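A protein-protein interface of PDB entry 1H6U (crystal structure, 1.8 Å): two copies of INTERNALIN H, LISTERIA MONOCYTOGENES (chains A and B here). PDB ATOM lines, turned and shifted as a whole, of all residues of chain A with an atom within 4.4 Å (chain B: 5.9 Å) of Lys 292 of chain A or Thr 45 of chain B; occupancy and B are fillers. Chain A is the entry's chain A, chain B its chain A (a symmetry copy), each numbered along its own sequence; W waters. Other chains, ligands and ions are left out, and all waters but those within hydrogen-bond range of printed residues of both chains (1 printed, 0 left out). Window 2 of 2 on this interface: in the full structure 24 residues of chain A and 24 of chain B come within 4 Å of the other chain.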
ATOM      1  N   ALA A 214     -18.123 -19.665   9.242  1.00  0.00           N
ATOM      2  CA  ALA A 214     -17.230 -18.962  10.181  1.00  0.00           C
ATOM      3  C   ALA A 214     -17.645 -17.532  10.473  1.00  0.00           C
ATOM      4  O   ALA A 214     -17.445 -17.029  11.599  1.00  0.00           O
ATOM      5  CB  ALA A 214     -15.776 -19.019   9.665  1.00  0.00           C
ATOM      6  N   ASN A 215     -18.276 -16.920   9.505  1.00  0.00           N
ATOM      7  CA  ASN A 215     -18.753 -15.574   9.659  1.00  0.00           C
ATOM      8  C   ASN A 215     -20.219 -15.355   9.914  1.00  0.00           C
ATOM      9  O   ASN A 215     -20.677 -14.236   9.808  1.00  0.00           O
ATOM     10  CB  ASN A 215     -18.309 -14.785   8.493  1.00  0.00           C
ATOM     11  CG  ASN A 215     -17.093 -13.999   8.830  1.00  0.00           C
ATOM     12  OD1 ASN A 215     -15.970 -14.549   9.133  1.00  0.00           O
ATOM     13  ND2 ASN A 215     -17.308 -12.670   8.887  1.00  0.00           N
ATOM     14  N   THR A 216     -20.954 -16.415  10.186  1.00  0.00           N
ATOM     15  CA  THR A 216     -22.354 -16.329  10.489  1.00  0.00           C
ATOM     16  C   THR A 216     -22.522 -15.858  11.941  1.00  0.00           C
ATOM     17  O   THR A 216     -22.331 -16.608  12.854  1.00  0.00           O
ATOM     18  CB  THR A 216     -22.946 -17.692  10.299  1.00  0.00           C
ATOM     19  OG1 THR A 216     -22.604 -18.181   8.998  1.00  0.00           O
ATOM     20  CG2 THR A 216     -24.440 -17.676  10.385  1.00  0.00           C
ATOM     21  N   SER A 217     -22.875 -14.592  12.134  1.00  0.00           N
ATOM     22  CA  SER A 217     -22.880 -13.970  13.466  1.00  0.00           C
ATOM     23  C   SER A 217     -24.070 -14.357  14.318  1.00  0.00           C
ATOM     24  O   SER A 217     -24.026 -14.097  15.506  1.00  0.00           O
ATOM     25  CB  SER A 217     -22.779 -12.440  13.375  1.00  0.00           C
ATOM     26  OG  SER A 217     -21.687 -12.067  12.561  1.00  0.00           O
ATOM     27  N   PHE A 291     -16.864 -21.530  16.041  1.00  0.00           N
ATOM     28  CA  PHE A 291     -17.448 -20.612  15.088  1.00  0.00           C
ATOM     29  C   PHE A 291     -17.538 -19.238  15.752  1.00  0.00           C
ATOM     30  O   PHE A 291     -16.952 -19.025  16.787  1.00  0.00           O
ATOM     31  CB  PHE A 291     -18.776 -21.148  14.605  1.00  0.00           C
ATOM     32  CG  PHE A 291     -18.639 -22.396  13.753  1.00  0.00           C
ATOM     33  CD1 PHE A 291     -18.283 -22.276  12.435  1.00  0.00           C
ATOM     34  CD2 PHE A 291     -18.759 -23.631  14.287  1.00  0.00           C
ATOM     35  CE1 PHE A 291     -18.101 -23.366  11.672  1.00  0.00           C
ATOM     36  CE2 PHE A 291     -18.645 -24.765  13.520  1.00  0.00           C
ATOM     37  CZ  PHE A 291     -18.287 -24.637  12.208  1.00  0.00           C
ATOM     38  N   LYS A 292     -18.259 -18.304  15.131  1.00  0.00           N
ATOM     39  CA  LYS A 292     -18.368 -16.947  15.642  1.00  0.00           C
ATOM     40  C   LYS A 292     -18.805 -16.930  17.092  1.00  0.00           C
ATOM     41  O   LYS A 292     -18.224 -16.211  17.885  1.00  0.00           O
ATOM     42  CB  LYS A 292     -19.316 -16.105  14.741  1.00  0.00           C
ATOM     43  CG  LYS A 292     -18.912 -14.659  14.444  1.00  0.00           C
ATOM     44  CD  LYS A 292     -17.497 -14.470  13.937  1.00  0.00           C
ATOM     45  CE  LYS A 292     -17.200 -13.043  13.578  1.00  0.00           C
ATOM     46  NZ  LYS A 292     -17.330 -12.645  12.119  1.00  0.00           N
ATOM     47  N   ASN A 293     -19.800 -17.698  17.465  1.00  0.00           N
ATOM     48  CA  ASN A 293     -20.327 -17.630  18.809  1.00  0.00           C
ATOM     49  C   ASN A 293     -19.879 -18.733  19.665  1.00  0.00           C
ATOM     50  O   ASN A 293     -19.329 -18.421  20.761  1.00  0.00           O
ATOM     51  CB  ASN A 293     -21.850 -17.579  18.817  1.00  0.00           C
ATOM     52  CG  ASN A 293     -22.343 -16.354  18.207  1.00  0.00           C
ATOM     53  OD1 ASN A 293     -21.904 -15.305  18.596  1.00  0.00           O
ATOM     54  ND2 ASN A 293     -23.202 -16.452  17.176  1.00  0.00           N
ATOM     55  N   THR A 294     -20.068 -19.975  19.209  1.00  0.00           N
ATOM     56  CA  THR A 294     -19.731 -21.176  19.988  1.00  0.00           C
ATOM     57  C   THR A 294     -18.834 -22.241  19.322  1.00  0.00           C
ATOM     58  O   THR A 294     -18.408 -22.110  18.191  1.00  0.00           O
ATOM     59  CB  THR A 294     -20.903 -21.855  20.399  1.00  0.00           C
ATOM     60  OG1 THR A 294     -21.694 -22.171  19.237  1.00  0.00           O
ATOM     61  CG2 THR A 294     -21.753 -20.918  21.257  1.00  0.00           C
ATOM     62  N   ALA B  25      -8.012  -8.637  13.443  1.00  0.00           N
ATOM     63  CA  ALA B  25      -9.158  -8.013  12.781  1.00  0.00           C
ATOM     64  C   ALA B  25      -8.660  -6.858  11.966  1.00  0.00           C
ATOM     65  O   ALA B  25      -9.295  -6.477  10.948  1.00  0.00           O
ATOM     66  CB  ALA B  25     -10.145  -7.573  13.805  1.00  0.00           C
ATOM     67  N   ILE B  43     -13.355  -2.130  11.486  1.00  0.00           N
ATOM     68  CA  ILE B  43     -13.618  -3.374  12.199  1.00  0.00           C
ATOM     69  C   ILE B  43     -15.117  -3.529  12.505  1.00  0.00           C
ATOM     70  O   ILE B  43     -15.690  -2.730  13.275  1.00  0.00           O
ATOM     71  CB  ILE B  43     -12.776  -3.461  13.468  1.00  0.00           C
ATOM     72  CG1 ILE B  43     -11.290  -3.482  13.148  1.00  0.00           C
ATOM     73  CG2 ILE B  43     -13.174  -4.683  14.305  1.00  0.00           C
ATOM     74  CD1 ILE B  43     -10.382  -3.630  14.358  1.00  0.00           C
ATOM     75  N   THR B  44     -15.753  -4.507  11.896  1.00  0.00           N
ATOM     76  CA  THR B  44     -17.161  -4.734  12.058  1.00  0.00           C
ATOM     77  C   THR B  44     -17.520  -5.905  12.947  1.00  0.00           C
ATOM     78  O   THR B  44     -18.636  -5.977  13.463  1.00  0.00           O
ATOM     79  CB  THR B  44     -17.914  -4.867  10.738  1.00  0.00           C
ATOM     80  OG1 THR B  44     -17.353  -5.949   9.975  1.00  0.00           O
ATOM     81  CG2 THR B  44     -17.772  -3.545   9.929  1.00  0.00           C
ATOM     82  N   THR B  45     -16.599  -6.835  13.116  1.00  0.00           N
ATOM     83  CA  THR B  45     -16.792  -7.924  14.070  1.00  0.00           C
ATOM     84  C   THR B  45     -15.511  -8.182  14.872  1.00  0.00           C
ATOM     85  O   THR B  45     -14.380  -7.967  14.437  1.00  0.00           O
ATOM     86  CB  THR B  45     -17.265  -9.255  13.439  1.00  0.00           C
ATOM     87  OG1 THR B  45     -16.256  -9.782  12.601  1.00  0.00           O
ATOM     88  CG2 THR B  45     -18.511  -9.074  12.567  1.00  0.00           C
ATOM     89  N   LEU B  46     -15.714  -8.596  16.123  1.00  0.00           N
ATOM     90  CA  LEU B  46     -14.608  -8.880  17.001  1.00  0.00           C
ATOM     91  C   LEU B  46     -14.979 -10.099  17.806  1.00  0.00           C
ATOM     92  O   LEU B  46     -15.944 -10.059  18.585  1.00  0.00           O
ATOM     93  CB  LEU B  46     -14.338  -7.735  17.936  1.00  0.00           C
ATOM     94  CG  LEU B  46     -13.073  -7.790  18.781  1.00  0.00           C
ATOM     95  CD1 LEU B  46     -11.873  -7.898  17.960  1.00  0.00           C
ATOM     96  CD2 LEU B  46     -12.968  -6.581  19.644  1.00  0.00           C
ATOM     97  N   SER B  47     -14.173 -11.159  17.725  1.00  0.00           N
ATOM     98  CA  SER B  47     -14.501 -12.420  18.369  1.00  0.00           C
ATOM     99  C   SER B  47     -13.324 -12.958  19.184  1.00  0.00           C
ATOM    100  O   SER B  47     -12.191 -12.917  18.722  1.00  0.00           O
ATOM    101  CB  SER B  47     -14.843 -13.496  17.322  1.00  0.00           C
ATOM    102  OG  SER B  47     -15.661 -12.870  16.330  1.00  0.00           O
ATOM    103  N   PHE B  49     -13.647 -15.955  21.813  1.00  0.00           N
ATOM    104  CA  PHE B  49     -14.195 -17.009  22.668  1.00  0.00           C
ATOM    105  C   PHE B  49     -13.032 -17.633  23.442  1.00  0.00           C
ATOM    106  O   PHE B  49     -12.016 -18.014  22.810  1.00  0.00           O
ATOM    107  CB  PHE B  49     -14.723 -18.110  21.762  1.00  0.00           C
ATOM    108  CG  PHE B  49     -15.042 -19.413  22.519  1.00  0.00           C
ATOM    109  CD1 PHE B  49     -16.200 -19.561  23.239  1.00  0.00           C
ATOM    110  CD2 PHE B  49     -14.133 -20.405  22.573  1.00  0.00           C
ATOM    111  CE1 PHE B  49     -16.445 -20.719  23.974  1.00  0.00           C
ATOM    112  CE2 PHE B  49     -14.362 -21.542  23.298  1.00  0.00           C
ATOM    113  CZ  PHE B  49     -15.515 -21.678  24.011  1.00  0.00           C
ATOM    114  N   ASN B  64     -17.964   1.318  14.133  1.00  0.00           N
ATOM    115  CA  ASN B  64     -18.759   0.570  13.195  1.00  0.00           C
ATOM    116  C   ASN B  64     -18.974  -0.900  13.570  1.00  0.00           C
ATOM    117  O   ASN B  64     -19.355  -1.695  12.736  1.00  0.00           O
ATOM    118  CB  ASN B  64     -18.150   0.686  11.863  1.00  0.00           C
ATOM    119  CG  ASN B  64     -18.362   2.104  11.263  1.00  0.00           C
ATOM    120  OD1 ASN B  64     -19.427   2.710  11.457  1.00  0.00           O
ATOM    121  ND2 ASN B  64     -17.376   2.583  10.498  1.00  0.00           N
ATOM    122  N   LEU B  65     -18.779  -1.199  14.837  1.00  0.00           N
ATOM    123  CA  LEU B  65     -18.831  -2.622  15.263  1.00  0.00           C
ATOM    124  C   LEU B  65     -20.252  -3.112  15.201  1.00  0.00           C
ATOM    125  O   LEU B  65     -21.201  -2.498  15.758  1.00  0.00           O
ATOM    126  CB  LEU B  65     -18.298  -2.734  16.643  1.00  0.00           C
ATOM    127  CG  LEU B  65     -18.080  -4.192  17.167  1.00  0.00           C
ATOM    128  CD1 LEU B  65     -16.948  -4.851  16.497  1.00  0.00           C
ATOM    129  CD2 LEU B  65     -17.822  -4.073  18.687  1.00  0.00           C
ATOM    130  N   ILE B  66     -20.419  -4.241  14.545  1.00  0.00           N
ATOM    131  CA  ILE B  66     -21.743  -4.855  14.432  1.00  0.00           C
ATOM    132  C   ILE B  66     -21.870  -6.076  15.331  1.00  0.00           C
ATOM    133  O   ILE B  66     -22.936  -6.354  15.863  1.00  0.00           O
ATOM    134  CB  ILE B  66     -21.950  -5.296  12.989  1.00  0.00           C
ATOM    135  CG1 ILE B  66     -21.823  -4.054  12.028  1.00  0.00           C
ATOM    136  CG2 ILE B  66     -23.308  -5.885  12.810  1.00  0.00           C
ATOM    137  CD1 ILE B  66     -21.810  -4.431  10.548  1.00  0.00           C
ATOM    138  N   GLY B  67     -20.795  -6.845  15.437  1.00  0.00           N
ATOM    139  CA  GLY B  67     -20.866  -8.073  16.240  1.00  0.00           C
ATOM    140  C   GLY B  67     -19.707  -8.211  17.188  1.00  0.00           C
ATOM    141  O   GLY B  67     -18.578  -7.961  16.798  1.00  0.00           O
ATOM    142  N   LEU B  68     -20.003  -8.532  18.469  1.00  0.00           N
ATOM    143  CA  LEU B  68     -18.960  -8.686  19.448  1.00  0.00           C
ATOM    144  C   LEU B  68     -19.227 -10.052  20.079  1.00  0.00           C
ATOM    145  O   LEU B  68     -20.320 -10.226  20.714  1.00  0.00           O
ATOM    146  CB  LEU B  68     -19.091  -7.588  20.471  1.00  0.00           C
ATOM    147  CG  LEU B  68     -18.029  -7.565  21.558  1.00  0.00           C
ATOM    148  CD1 LEU B  68     -16.626  -7.510  20.962  1.00  0.00           C
ATOM    149  CD2 LEU B  68     -18.384  -6.475  22.524  1.00  0.00           C
ATOM    150  N   GLU B  69     -18.272 -10.974  19.952  1.00  0.00           N
ATOM    151  CA  GLU B  69     -18.495 -12.327  20.447  1.00  0.00           C
ATOM    152  C   GLU B  69     -17.402 -12.684  21.390  1.00  0.00           C
ATOM    153  O   GLU B  69     -16.259 -12.920  20.957  1.00  0.00           O
ATOM    154  CB  GLU B  69     -18.543 -13.305  19.273  1.00  0.00           C
ATOM    155  CG  GLU B  69     -19.661 -12.921  18.293  1.00  0.00           C
ATOM    156  CD  GLU B  69     -19.233 -12.057  17.119  1.00  0.00           C
ATOM    157  OE1 GLU B  69     -18.021 -11.843  16.927  1.00  0.00           O
ATOM    158  OE2 GLU B  69     -20.173 -11.535  16.422  1.00  0.00           O
ATOM    159  N   GLU B  89     -25.286  -7.753  17.257  1.00  0.00           N
ATOM    160  CA  GLU B  89     -25.134  -9.084  17.846  1.00  0.00           C
ATOM    161  C   GLU B  89     -24.151  -8.980  18.944  1.00  0.00           C
ATOM    162  O   GLU B  89     -23.047  -8.552  18.714  1.00  0.00           O
ATOM    163  CB  GLU B  89     -24.730 -10.152  16.813  1.00  0.00           C
ATOM    164  CG  GLU B  89     -24.807 -11.542  17.423  1.00  0.00           C
ATOM    165  CD  GLU B  89     -23.484 -12.228  17.723  1.00  0.00           C
ATOM    166  OE1 GLU B  89     -22.435 -11.801  17.190  1.00  0.00           O
ATOM    167  OE2 GLU B  89     -23.536 -13.278  18.465  1.00  0.00           O
ATOM    168  N   GLU B  91     -22.645 -11.280  22.144  1.00  0.00           N
ATOM    169  CA  GLU B  91     -22.463 -12.647  22.725  1.00  0.00           C
ATOM    170  C   GLU B  91     -21.559 -12.508  23.938  1.00  0.00           C
ATOM    171  O   GLU B  91     -20.317 -12.394  23.781  1.00  0.00           O
ATOM    172  CB  GLU B  91     -21.903 -13.584  21.658  1.00  0.00           C
ATOM    173  CG  GLU B  91     -21.299 -14.879  22.147  1.00  0.00           C
ATOM    174  CD  GLU B  91     -22.347 -15.672  22.812  1.00  0.00           C
ATOM    175  OE1 GLU B  91     -22.556 -15.425  23.978  1.00  0.00           O
ATOM    176  OE2 GLU B  91     -22.985 -16.601  22.176  1.00  0.00           O
HETATM  177  O   HOH W   1     -17.720 -15.835  21.551  1.00  0.00           O
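Of the 15 printed residues of chain B, 5 touch a printed residue of chain A. Among the printed residues, 7 pairs touch across the chains.
Printed residues of chain B within 4 Å of Ser 217 of chain A: Glu 89. Of chain B, only Thr 45 (3.1 Å), Ser 47 (3.2 Å) and Glu 69 (3.2 Å) come within 4 Å of Lys 292 of chain A. Of the printed residues of chain B, Asn 293 of chain A touches Glu 69, Glu 89 and Glu 91. Thr 294 of chain A touches none of the printed residues of chain B. Thr 45 of chain B touches one residue of chain A. Printed residues of chain A within 4 Å of Ser 47 of chain B: Lys 292. Phe 49 of chain B touches none of the printed residues of chain A. Printed residues of chain A within 4 Å of Glu 69 of chain B: Lys 292 (3.2 Å) and Asn 293 (3.3 Å). Of the printed residues of chain A, Glu 91 of chain B touches Asn 293 (3.5 Å). The nearest residue of chain B that does not touch Lys 292 of chain A is Glu 89 of chain B (5.3 Å). The nearest printed residue of chain A that does not touch Thr 45 of chain B is Ser 217 of chain A (4.4 Å).
NZ of Lys 292 of chain A lies close to ND2 of Asn 215 of chain A (3.2 Å). The side-chain amide nitrogen (ND2) of Asn 293 of chain A sits at hydrogen-bond distance from the backbone carbonyl oxygen (O) of Ser 217 of chain A. O of Leu 46 of chain B lies within hydrogen-bond range of N of Glu 69 of chain B, 2.9 Å away. N of Leu 68 of chain B is in hydrogen-bond range of O of Glu 89 of chain B (3.1 Å). The backbone carbonyl oxygen of Leu 68 of chain B is in hydrogen-bond range of the backbone NH of Glu 91 of chain B, at 2.9 Å. The side-chain carboxylate (OE2) of Glu 69 of chain B sits close to the side-chain carboxylate (OE1) of Glu 89 of chain B, 2.4 Å away.
The side-chain amino group (NZ) of Lys 292 of chain A lies within hydrogen-bond range of the side-chain hydroxyl (OG1) of Thr 45 of chain B. OD1 of Asn 293 of chain A sits close to OE2 of Glu 89 of chain B. The side-chain carboxylate (OE2) of Glu 89 of chain B lies close to the backbone carbonyl oxygen (O) of Ser 217 of chain A, 3.1 Å away.
No position is printed for both chains.
Among the printed residues, pairs that only touch across the chains: Lys 292 of chain A with Ser 47 of chain B (3.2 Å), Lys 292 of chain A with Glu 69 of chain B (3.2 Å), Asn 293 of chain A with Glu 69 of chain B (3.3 Å) and Asn 293 of chain A with Glu 91 of chain B (3.5 Å).
Water W1 bridges the backbone carbonyl oxygen (O) of Asn 293 of chain A (3.1 Å) and the backbone carbonyl oxygen (O) of Glu 69 of chain B (3.3 Å).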
